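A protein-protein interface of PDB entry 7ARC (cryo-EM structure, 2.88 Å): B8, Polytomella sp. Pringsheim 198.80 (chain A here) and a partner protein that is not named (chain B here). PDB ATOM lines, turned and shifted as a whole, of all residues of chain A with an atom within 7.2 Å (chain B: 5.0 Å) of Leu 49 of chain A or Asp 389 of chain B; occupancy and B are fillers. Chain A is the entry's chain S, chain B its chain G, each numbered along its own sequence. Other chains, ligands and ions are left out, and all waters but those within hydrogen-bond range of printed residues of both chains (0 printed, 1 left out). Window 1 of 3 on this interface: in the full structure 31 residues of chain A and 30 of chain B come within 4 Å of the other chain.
NH2 of Arg 51 of chain A lies within hydrogen-bond range of OH of Tyr 394 of chain B, at 3.2 Å.
The backbone carbonyl oxygen of Asp 532 of chain B lies within hydrogen-bond range of the guanidinium group of Arg 51 of chain A, at 3.0 Å.
The backbone NH of Ile 48 of chain A is in hydrogen-bond range of the side-chain carboxylate of Asp 389 of chain B (2.9 Å).
O of Asp 389 of chain B is in hydrogen-bond range of N of Val 50 of chain A.
NZ of Lys 40 of chain A lies within salt-bridge range of OD1 of Asp 389 of chain B (3.6 Å).
NH1 of Arg 51 of chain A lies within hydrogen-bond range of O of Asp 389 of chain B.
The guanidinium group (NH2) of Arg 51 of chain A lies within hydrogen-bond range of the backbone carbonyl oxygen (O) of Ala 388 of chain B, at 2.5 Å.
The guanidinium group (NH2) of Arg 51 of chain A sits at hydrogen-bond distance from the backbone carbonyl oxygen (O) of Leu 531 of chain B, 2.8 Å away.
OE1 of Glu 13 of chain A is in salt-bridge range of NH2 of Arg 63 of chain A (3.6 Å).
The side-chain hydroxyl (OH) of Tyr 394 of chain B lies within hydrogen-bond range of the side-chain carboxylate (OD1) of Asp 532 of chain B, 2.8 Å away.
The backbone NH (N) of Leu 14 of chain A is in hydrogen-bond range of the backbone carbonyl oxygen (O) of Pro 47 of chain A (3.0 Å).
O of Leu 14 of chain A is in hydrogen-bond range of N of Leu 49 of chain A, at 2.7 Å.
O of Leu 46 of chain A sits at hydrogen-bond distance from NZ of Lys 40 of chain A, at 2.8 Å.
N of Ile 16 of chain A lies within hydrogen-bond range of O of Leu 49 of chain A (2.7 Å).
Gly 534 of chain B touches Glu 13 of chain A (CA to OE2, 3.9 Å).
CB of Asp 389 of chain B touches OH of Tyr 36 of chain A (3.3 Å).
Tyr 36 of chain A touches Val 390 of chain B.
CD1 of Tyr 673 of chain B touches OH of Tyr 36 of chain A, at 3.4 Å.
Leu 46 of chain A touches Asp 389 of chain B.
OD2 of Asp 389 of chain B touches C of Pro 47 of chain A, 3.8 Å away.
O of Ala 388 of chain B touches CD2 of Leu 49 of chain A, at 3.5 Å.
CA of Leu 49 of chain A touches O of Asp 389 of chain B (3.5 Å).
Glu 52 of chain A touches Arg 391 of chain B.
Leu 49 of chain A touches just these residues of chain B: Ala 388 and Asp 389.
Printed residues of chain B within 4 Å of Glu 13 of chain A: Gly 534 (3.9 Å).
Printed residues of chain B within 4 Å of Glu 52 of chain A: Arg 391.
Of the printed residues of chain A, Arg 391 of chain B touches Glu 52 (3.9 Å).
Thr 61 of chain A touches none of the printed residues of chain B.
The nearest printed residue of chain A that does not touch Leu 531 of chain B is Leu 49 of chain A (4.9 Å).
Hydrophobic or aromatic side chains of chain B that line the printed part of chain A: Ala 388, Val 390, Tyr 394 and Tyr 673.
Of the 20 printed residues of chain A, 10 touch a printed residue of chain B.
Among the printed residues, 17 pairs touch across the chains.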
ATOM      1  N   GLU A  13      -0.287  11.862 -31.925  1.00  0.00           N
ATOM      2  CA  GLU A  13      -0.458  12.566 -30.668  1.00  0.00           C
ATOM      3  C   GLU A  13      -1.652  13.501 -30.787  1.00  0.00           C
ATOM      4  O   GLU A  13      -2.032  13.912 -31.885  1.00  0.00           O
ATOM      5  CB  GLU A  13       0.831  13.321 -30.347  1.00  0.00           C
ATOM      6  CG  GLU A  13       0.910  14.055 -29.049  1.00  0.00           C
ATOM      7  CD  GLU A  13       2.272  14.687 -28.896  1.00  0.00           C
ATOM      8  OE1 GLU A  13       3.087  14.560 -29.830  1.00  0.00           O
ATOM      9  OE2 GLU A  13       2.555  15.274 -27.842  1.00  0.00           O
ATOM     10  N   LEU A  14      -2.248  13.830 -29.642  1.00  0.00           N
ATOM     11  CA  LEU A  14      -3.382  14.742 -29.586  1.00  0.00           C
ATOM     12  C   LEU A  14      -3.123  15.799 -28.523  1.00  0.00           C
ATOM     13  O   LEU A  14      -2.803  15.462 -27.379  1.00  0.00           O
ATOM     14  CB  LEU A  14      -4.677  13.981 -29.292  1.00  0.00           C
ATOM     15  CG  LEU A  14      -5.966  14.781 -29.141  1.00  0.00           C
ATOM     16  CD1 LEU A  14      -6.292  15.492 -30.437  1.00  0.00           C
ATOM     17  CD2 LEU A  14      -7.105  13.861 -28.743  1.00  0.00           C
ATOM     18  N   ARG A  15      -3.258  17.069 -28.894  1.00  0.00           N
ATOM     19  CA  ARG A  15      -3.031  18.185 -27.985  1.00  0.00           C
ATOM     20  C   ARG A  15      -4.333  18.941 -27.760  1.00  0.00           C
ATOM     21  O   ARG A  15      -5.038  19.264 -28.721  1.00  0.00           O
ATOM     22  CB  ARG A  15      -1.968  19.133 -28.535  1.00  0.00           C
ATOM     23  CG  ARG A  15      -0.578  18.536 -28.603  1.00  0.00           C
ATOM     24  CD  ARG A  15       0.478  19.612 -28.447  1.00  0.00           C
ATOM     25  NE  ARG A  15       0.499  20.521 -29.586  1.00  0.00           N
ATOM     26  CZ  ARG A  15       1.215  20.329 -30.685  1.00  0.00           C
ATOM     27  NH1 ARG A  15       2.032  19.295 -30.806  1.00  0.00           N
ATOM     28  NH2 ARG A  15       1.124  21.207 -31.680  1.00  0.00           N
ATOM     29  N   ILE A  16      -4.651  19.220 -26.500  1.00  0.00           N
ATOM     30  CA  ILE A  16      -5.829  20.003 -26.137  1.00  0.00           C
ATOM     31  C   ILE A  16      -5.341  21.244 -25.403  1.00  0.00           C
ATOM     32  O   ILE A  16      -5.021  21.184 -24.210  1.00  0.00           O
ATOM     33  CB  ILE A  16      -6.814  19.204 -25.279  1.00  0.00           C
ATOM     34  CG1 ILE A  16      -7.347  18.007 -26.063  1.00  0.00           C
ATOM     35  CG2 ILE A  16      -7.965  20.089 -24.840  1.00  0.00           C
ATOM     36  CD1 ILE A  16      -8.119  17.025 -25.222  1.00  0.00           C
ATOM     37  N   THR A  17      -5.275  22.371 -26.103  1.00  0.00           N
ATOM     38  CA  THR A  17      -4.908  23.642 -25.496  1.00  0.00           C
ATOM     39  C   THR A  17      -6.157  24.386 -25.038  1.00  0.00           C
ATOM     40  O   THR A  17      -7.162  24.429 -25.753  1.00  0.00           O
ATOM     41  CB  THR A  17      -4.115  24.502 -26.485  1.00  0.00           C
ATOM     42  OG1 THR A  17      -2.813  23.936 -26.674  1.00  0.00           O
ATOM     43  CG2 THR A  17      -3.966  25.927 -25.971  1.00  0.00           C
ATOM     44  N   LEU A  18      -6.098  24.959 -23.839  1.00  0.00           N
ATOM     45  CA  LEU A  18      -7.261  25.628 -23.270  1.00  0.00           C
ATOM     46  C   LEU A  18      -6.788  26.668 -22.263  1.00  0.00           C
ATOM     47  O   LEU A  18      -5.637  26.653 -21.825  1.00  0.00           O
ATOM     48  CB  LEU A  18      -8.228  24.628 -22.622  1.00  0.00           C
ATOM     49  CG  LEU A  18      -7.852  23.970 -21.294  1.00  0.00           C
ATOM     50  CD1 LEU A  18      -9.077  23.335 -20.670  1.00  0.00           C
ATOM     51  CD2 LEU A  18      -6.763  22.937 -21.477  1.00  0.00           C
ATOM     52  N   TYR A  36     -12.084  13.224 -21.150  1.00  0.00           N
ATOM     53  CA  TYR A  36     -10.684  12.821 -21.243  1.00  0.00           C
ATOM     54  C   TYR A  36     -10.475  11.413 -20.693  1.00  0.00           C
ATOM     55  O   TYR A  36      -9.703  10.629 -21.258  1.00  0.00           O
ATOM     56  CB  TYR A  36      -9.791  13.825 -20.515  1.00  0.00           C
ATOM     57  CG  TYR A  36      -8.428  13.286 -20.139  1.00  0.00           C
ATOM     58  CD1 TYR A  36      -7.394  13.267 -21.062  1.00  0.00           C
ATOM     59  CD2 TYR A  36      -8.173  12.807 -18.863  1.00  0.00           C
ATOM     60  CE1 TYR A  36      -6.148  12.779 -20.730  1.00  0.00           C
ATOM     61  CE2 TYR A  36      -6.931  12.316 -18.523  1.00  0.00           C
ATOM     62  CZ  TYR A  36      -5.922  12.305 -19.460  1.00  0.00           C
ATOM     63  OH  TYR A  36      -4.682  11.820 -19.124  1.00  0.00           O
ATOM     64  N   LYS A  40      -9.035   8.318 -22.881  1.00  0.00           N
ATOM     65  CA  LYS A  40      -7.834   7.622 -22.433  1.00  0.00           C
ATOM     66  C   LYS A  40      -8.099   6.138 -22.225  1.00  0.00           C
ATOM     67  O   LYS A  40      -7.244   5.303 -22.535  1.00  0.00           O
ATOM     68  CB  LYS A  40      -7.307   8.259 -21.148  1.00  0.00           C
ATOM     69  CG  LYS A  40      -6.034   7.624 -20.623  1.00  0.00           C
ATOM     70  CD  LYS A  40      -4.887   7.779 -21.587  1.00  0.00           C
ATOM     71  CE  LYS A  40      -4.437   9.208 -21.680  1.00  0.00           C
ATOM     72  NZ  LYS A  40      -3.269   9.315 -22.588  1.00  0.00           N
ATOM     73  N   ASN A  43      -8.018   4.618 -25.596  1.00  0.00           N
ATOM     74  CA  ASN A  43      -6.708   4.737 -26.236  1.00  0.00           C
ATOM     75  C   ASN A  43      -5.649   4.888 -25.155  1.00  0.00           C
ATOM     76  O   ASN A  43      -5.199   6.003 -24.859  1.00  0.00           O
ATOM     77  CB  ASN A  43      -6.681   5.922 -27.201  1.00  0.00           C
ATOM     78  CG  ASN A  43      -7.649   5.753 -28.348  1.00  0.00           C
ATOM     79  OD1 ASN A  43      -7.493   4.863 -29.181  1.00  0.00           O
ATOM     80  ND2 ASN A  43      -8.670   6.599 -28.386  1.00  0.00           N
ATOM     81  N   PRO A  44      -5.233   3.782 -24.537  1.00  0.00           N
ATOM     82  CA  PRO A  44      -4.301   3.891 -23.402  1.00  0.00           C
ATOM     83  C   PRO A  44      -2.947   4.476 -23.764  1.00  0.00           C
ATOM     84  O   PRO A  44      -2.446   5.360 -23.057  1.00  0.00           O
ATOM     85  CB  PRO A  44      -4.185   2.436 -22.931  1.00  0.00           C
ATOM     86  CG  PRO A  44      -5.452   1.799 -23.383  1.00  0.00           C
ATOM     87  CD  PRO A  44      -5.686   2.396 -24.731  1.00  0.00           C
ATOM     88  N   LEU A  45      -2.334   4.006 -24.851  1.00  0.00           N
ATOM     89  CA  LEU A  45      -0.975   4.405 -25.191  1.00  0.00           C
ATOM     90  C   LEU A  45      -0.903   5.706 -25.980  1.00  0.00           C
ATOM     91  O   LEU A  45       0.197   6.233 -26.169  1.00  0.00           O
ATOM     92  CB  LEU A  45      -0.295   3.290 -25.985  1.00  0.00           C
ATOM     93  CG  LEU A  45      -0.063   1.985 -25.221  1.00  0.00           C
ATOM     94  CD1 LEU A  45       0.488   0.916 -26.141  1.00  0.00           C
ATOM     95  CD2 LEU A  45       0.856   2.198 -24.037  1.00  0.00           C
ATOM     96  N   LEU A  46      -2.030   6.230 -26.443  1.00  0.00           N
ATOM     97  CA  LEU A  46      -2.024   7.495 -27.169  1.00  0.00           C
ATOM     98  C   LEU A  46      -1.718   8.649 -26.219  1.00  0.00           C
ATOM     99  O   LEU A  46      -2.358   8.764 -25.169  1.00  0.00           O
ATOM    100  CB  LEU A  46      -3.371   7.716 -27.849  1.00  0.00           C
ATOM    101  CG  LEU A  46      -3.575   9.062 -28.544  1.00  0.00           C
ATOM    102  CD1 LEU A  46      -2.772   9.118 -29.826  1.00  0.00           C
ATOM    103  CD2 LEU A  46      -5.046   9.303 -28.818  1.00  0.00           C
ATOM    104  N   PRO A  47      -0.753   9.513 -26.542  1.00  0.00           N
ATOM    105  CA  PRO A  47      -0.517  10.721 -25.738  1.00  0.00           C
ATOM    106  C   PRO A  47      -1.547  11.798 -26.045  1.00  0.00           C
ATOM    107  O   PRO A  47      -1.528  12.411 -27.117  1.00  0.00           O
ATOM    108  CB  PRO A  47       0.900  11.144 -26.162  1.00  0.00           C
ATOM    109  CG  PRO A  47       1.457   9.948 -26.916  1.00  0.00           C
ATOM    110  CD  PRO A  47       0.265   9.375 -27.590  1.00  0.00           C
ATOM    111  N   ILE A  48      -2.450  12.033 -25.098  1.00  0.00           N
ATOM    112  CA  ILE A  48      -3.404  13.136 -25.160  1.00  0.00           C
ATOM    113  C   ILE A  48      -2.929  14.205 -24.183  1.00  0.00           C
ATOM    114  O   ILE A  48      -3.097  14.066 -22.971  1.00  0.00           O
ATOM    115  CB  ILE A  48      -4.829  12.675 -24.843  1.00  0.00           C
ATOM    116  CG1 ILE A  48      -5.199  11.456 -25.685  1.00  0.00           C
ATOM    117  CG2 ILE A  48      -5.816  13.807 -25.067  1.00  0.00           C
ATOM    118  CD1 ILE A  48      -6.560  10.893 -25.363  1.00  0.00           C
ATOM    119  N   LEU A  49      -2.352  15.285 -24.699  1.00  0.00           N
ATOM    120  CA  LEU A  49      -1.724  16.302 -23.863  1.00  0.00           C
ATOM    121  C   LEU A  49      -2.692  17.452 -23.631  1.00  0.00           C
ATOM    122  O   LEU A  49      -3.142  18.091 -24.587  1.00  0.00           O
ATOM    123  CB  LEU A  49      -0.443  16.858 -24.476  1.00  0.00           C
ATOM    124  CG  LEU A  49       0.637  16.048 -25.169  1.00  0.00           C
ATOM    125  CD1 LEU A  49       1.571  17.075 -25.768  1.00  0.00           C
ATOM    126  CD2 LEU A  49       1.364  15.125 -24.218  1.00  0.00           C
ATOM    127  N   VAL A  50      -3.004  17.715 -22.370  1.00  0.00           N
ATOM    128  CA  VAL A  50      -3.854  18.836 -21.997  1.00  0.00           C
ATOM    129  C   VAL A  50      -2.932  19.905 -21.429  1.00  0.00           C
ATOM    130  O   VAL A  50      -2.345  19.730 -20.356  1.00  0.00           O
ATOM    131  CB  VAL A  50      -4.925  18.418 -20.983  1.00  0.00           C
ATOM    132  CG1 VAL A  50      -5.867  19.564 -20.704  1.00  0.00           C
ATOM    133  CG2 VAL A  50      -5.690  17.213 -21.493  1.00  0.00           C
ATOM    134  N   ARG A  51      -2.807  21.017 -22.146  1.00  0.00           N
ATOM    135  CA  ARG A  51      -1.910  22.102 -21.782  1.00  0.00           C
ATOM    136  C   ARG A  51      -2.715  23.383 -21.623  1.00  0.00           C
ATOM    137  O   ARG A  51      -3.585  23.682 -22.444  1.00  0.00           O
ATOM    138  CB  ARG A  51      -0.821  22.293 -22.839  1.00  0.00           C
ATOM    139  CG  ARG A  51       0.120  21.109 -22.975  1.00  0.00           C
ATOM    140  CD  ARG A  51       0.955  20.894 -21.731  1.00  0.00           C
ATOM    141  NE  ARG A  51       1.834  19.742 -21.877  1.00  0.00           N
ATOM    142  CZ  ARG A  51       1.542  18.520 -21.457  1.00  0.00           C
ATOM    143  NH1 ARG A  51       0.397  18.250 -20.859  1.00  0.00           N
ATOM    144  NH2 ARG A  51       2.419  17.540 -21.652  1.00  0.00           N
ATOM    145  N   GLU A  52      -2.420  24.140 -20.572  1.00  0.00           N
ATOM    146  CA  GLU A  52      -3.268  25.255 -20.183  1.00  0.00           C
ATOM    147  C   GLU A  52      -2.436  26.461 -19.773  1.00  0.00           C
ATOM    148  O   GLU A  52      -1.353  26.319 -19.200  1.00  0.00           O
ATOM    149  CB  GLU A  52      -4.207  24.832 -19.047  1.00  0.00           C
ATOM    150  CG  GLU A  52      -3.512  24.564 -17.723  1.00  0.00           C
ATOM    151  CD  GLU A  52      -2.964  23.149 -17.628  1.00  0.00           C
ATOM    152  OE1 GLU A  52      -2.854  22.476 -18.672  1.00  0.00           O
ATOM    153  OE2 GLU A  52      -2.644  22.706 -16.508  1.00  0.00           O
ATOM    154  N   THR A  61      -5.453  20.115 -31.490  1.00  0.00           N
ATOM    155  CA  THR A  61      -4.457  19.800 -32.504  1.00  0.00           C
ATOM    156  C   THR A  61      -4.179  18.305 -32.519  1.00  0.00           C
ATOM    157  O   THR A  61      -4.003  17.691 -31.463  1.00  0.00           O
ATOM    158  CB  THR A  61      -3.154  20.562 -32.244  1.00  0.00           C
ATOM    159  OG1 THR A  61      -3.439  21.952 -32.051  1.00  0.00           O
ATOM    160  CG2 THR A  61      -2.192  20.400 -33.410  1.00  0.00           C
ATOM    161  N   ARG A  63      -1.620  15.440 -34.394  1.00  0.00           N
ATOM    162  CA  ARG A  63      -0.431  15.194 -35.198  1.00  0.00           C
ATOM    163  C   ARG A  63      -0.538  13.816 -35.840  1.00  0.00           C
ATOM    164  O   ARG A  63      -0.667  12.808 -35.139  1.00  0.00           O
ATOM    165  CB  ARG A  63       0.839  15.311 -34.357  1.00  0.00           C
ATOM    166  CG  ARG A  63       2.104  15.307 -35.190  1.00  0.00           C
ATOM    167  CD  ARG A  63       3.352  15.266 -34.336  1.00  0.00           C
ATOM    168  NE  ARG A  63       3.697  13.912 -33.925  1.00  0.00           N
ATOM    169  CZ  ARG A  63       4.056  13.579 -32.694  1.00  0.00           C
ATOM    170  NH1 ARG A  63       4.185  14.490 -31.746  1.00  0.00           N
ATOM    171  NH2 ARG A  63       4.309  12.305 -32.413  1.00  0.00           N
ATOM    172  N   SER B 387       3.726   9.428 -18.200  1.00  0.00           N
ATOM    173  CA  SER B 387       2.715  10.112 -18.992  1.00  0.00           C
ATOM    174  C   SER B 387       2.920  11.619 -18.931  1.00  0.00           C
ATOM    175  O   SER B 387       3.138  12.188 -17.858  1.00  0.00           O
ATOM    176  CB  SER B 387       1.317   9.750 -18.498  1.00  0.00           C
ATOM    177  OG  SER B 387       1.051   8.372 -18.685  1.00  0.00           O
ATOM    178  N   ALA B 388       2.848  12.264 -20.091  1.00  0.00           N
ATOM    179  CA  ALA B 388       2.882  13.714 -20.193  1.00  0.00           C
ATOM    180  C   ALA B 388       1.495  14.299 -20.410  1.00  0.00           C
ATOM    181  O   ALA B 388       1.375  15.472 -20.774  1.00  0.00           O
ATOM    182  CB  ALA B 388       3.812  14.139 -21.328  1.00  0.00           C
ATOM    183  N   ASP B 389       0.450  13.501 -20.190  1.00  0.00           N
ATOM    184  CA  ASP B 389      -0.899  13.891 -20.584  1.00  0.00           C
ATOM    185  C   ASP B 389      -1.409  15.082 -19.785  1.00  0.00           C
ATOM    186  O   ASP B 389      -1.900  16.059 -20.360  1.00  0.00           O
ATOM    187  CB  ASP B 389      -1.840  12.701 -20.438  1.00  0.00           C
ATOM    188  CG  ASP B 389      -1.497  11.584 -21.387  1.00  0.00           C
ATOM    189  OD1 ASP B 389      -0.414  10.986 -21.233  1.00  0.00           O
ATOM    190  OD2 ASP B 389      -2.292  11.327 -22.311  1.00  0.00           O
ATOM    191  N   VAL B 390      -1.297  15.032 -18.462  1.00  0.00           N
ATOM    192  CA  VAL B 390      -1.812  16.087 -17.601  1.00  0.00           C
ATOM    193  C   VAL B 390      -0.653  16.704 -16.832  1.00  0.00           C
ATOM    194  O   VAL B 390       0.186  15.990 -16.271  1.00  0.00           O
ATOM    195  CB  VAL B 390      -2.911  15.566 -16.655  1.00  0.00           C
ATOM    196  CG1 VAL B 390      -4.091  15.064 -17.462  1.00  0.00           C
ATOM    197  CG2 VAL B 390      -2.390  14.453 -15.774  1.00  0.00           C
ATOM    198  N   ARG B 391      -0.599  18.035 -16.835  1.00  0.00           N
ATOM    199  CA  ARG B 391       0.501  18.754 -16.206  1.00  0.00           C
ATOM    200  C   ARG B 391       0.523  18.558 -14.697  1.00  0.00           C
ATOM    201  O   ARG B 391       1.599  18.485 -14.094  1.00  0.00           O
ATOM    202  CB  ARG B 391       0.393  20.232 -16.563  1.00  0.00           C
ATOM    203  CG  ARG B 391       1.504  21.100 -16.044  1.00  0.00           C
ATOM    204  CD  ARG B 391       1.333  22.516 -16.555  1.00  0.00           C
ATOM    205  NE  ARG B 391       2.332  23.420 -16.003  1.00  0.00           N
ATOM    206  CZ  ARG B 391       3.537  23.601 -16.519  1.00  0.00           C
ATOM    207  NH1 ARG B 391       3.961  22.883 -17.544  1.00  0.00           N
ATOM    208  NH2 ARG B 391       4.337  24.520 -15.990  1.00  0.00           N
ATOM    209  N   TYR B 394       2.960  15.706 -13.044  1.00  0.00           N
ATOM    210  CA  TYR B 394       4.417  15.677 -12.963  1.00  0.00           C
ATOM    211  C   TYR B 394       5.037  16.990 -12.495  1.00  0.00           C
ATOM    212  O   TYR B 394       6.256  17.153 -12.607  1.00  0.00           O
ATOM    213  CB  TYR B 394       5.029  15.289 -14.312  1.00  0.00           C
ATOM    214  CG  TYR B 394       4.543  16.102 -15.490  1.00  0.00           C
ATOM    215  CD1 TYR B 394       5.113  17.333 -15.783  1.00  0.00           C
ATOM    216  CD2 TYR B 394       3.533  15.636 -16.316  1.00  0.00           C
ATOM    217  CE1 TYR B 394       4.684  18.081 -16.853  1.00  0.00           C
ATOM    218  CE2 TYR B 394       3.098  16.380 -17.393  1.00  0.00           C
ATOM    219  CZ  TYR B 394       3.679  17.601 -17.655  1.00  0.00           C
ATOM    220  OH  TYR B 394       3.253  18.351 -18.724  1.00  0.00           O
ATOM    221  N   LEU B 531       8.564  16.706 -20.797  1.00  0.00           N
ATOM    222  CA  LEU B 531       7.177  16.300 -20.594  1.00  0.00           C
ATOM    223  C   LEU B 531       6.208  17.338 -21.146  1.00  0.00           C
ATOM    224  O   LEU B 531       5.178  16.985 -21.729  1.00  0.00           O
ATOM    225  CB  LEU B 531       6.916  16.057 -19.110  1.00  0.00           C
ATOM    226  CG  LEU B 531       7.561  14.808 -18.511  1.00  0.00           C
ATOM    227  CD1 LEU B 531       7.800  14.991 -17.027  1.00  0.00           C
ATOM    228  CD2 LEU B 531       6.694  13.592 -18.768  1.00  0.00           C
ATOM    229  N   ASP B 532       6.516  18.623 -20.969  1.00  0.00           N
ATOM    230  CA  ASP B 532       5.616  19.676 -21.427  1.00  0.00           C
ATOM    231  C   ASP B 532       5.495  19.684 -22.945  1.00  0.00           C
ATOM    232  O   ASP B 532       4.387  19.752 -23.486  1.00  0.00           O
ATOM    233  CB  ASP B 532       6.095  21.034 -20.921  1.00  0.00           C
ATOM    234  CG  ASP B 532       5.830  21.229 -19.447  1.00  0.00           C
ATOM    235  OD1 ASP B 532       4.951  20.528 -18.903  1.00  0.00           O
ATOM    236  OD2 ASP B 532       6.491  22.088 -18.829  1.00  0.00           O
ATOM    237  N   ILE B 533       6.626  19.626 -23.652  1.00  0.00           N
ATOM    238  CA  ILE B 533       6.563  19.676 -25.109  1.00  0.00           C
ATOM    239  C   ILE B 533       5.941  18.402 -25.669  1.00  0.00           C
ATOM    240  O   ILE B 533       5.322  18.425 -26.737  1.00  0.00           O
ATOM    241  CB  ILE B 533       7.953  19.935 -25.714  1.00  0.00           C
ATOM    242  CG1 ILE B 533       8.916  18.804 -25.368  1.00  0.00           C
ATOM    243  CG2 ILE B 533       8.498  21.267 -25.234  1.00  0.00           C
ATOM    244  CD1 ILE B 533      10.214  18.873 -26.119  1.00  0.00           C
ATOM    245  N   GLY B 534       6.099  17.279 -24.976  1.00  0.00           N
ATOM    246  CA  GLY B 534       5.550  16.025 -25.449  1.00  0.00           C
ATOM    247  C   GLY B 534       6.630  15.135 -26.018  1.00  0.00           C
ATOM    248  O   GLY B 534       6.432  14.466 -27.036  1.00  0.00           O
ATOM    249  N   TYR B 673      -7.044  10.898 -15.184  1.00  0.00           N
ATOM    250  CA  TYR B 673      -5.965  10.141 -15.810  1.00  0.00           C
ATOM    251  C   TYR B 673      -5.899   8.722 -15.259  1.00  0.00           C
ATOM    252  O   TYR B 673      -5.797   7.750 -16.019  1.00  0.00           O
ATOM    253  CB  TYR B 673      -4.633  10.863 -15.605  1.00  0.00           C
ATOM    254  CG  TYR B 673      -3.426   9.989 -15.857  1.00  0.00           C
ATOM    255  CD1 TYR B 673      -3.074   9.618 -17.148  1.00  0.00           C
ATOM    256  CD2 TYR B 673      -2.648   9.527 -14.808  1.00  0.00           C
ATOM    257  CE1 TYR B 673      -1.978   8.818 -17.385  1.00  0.00           C
ATOM    258  CE2 TYR B 673      -1.550   8.724 -15.035  1.00  0.00           C
ATOM    259  CZ  TYR B 673      -1.221   8.373 -16.324  1.00  0.00           C
ATOM    260  OH  TYR B 673      -0.127   7.574 -16.555  1.00  0.00           O
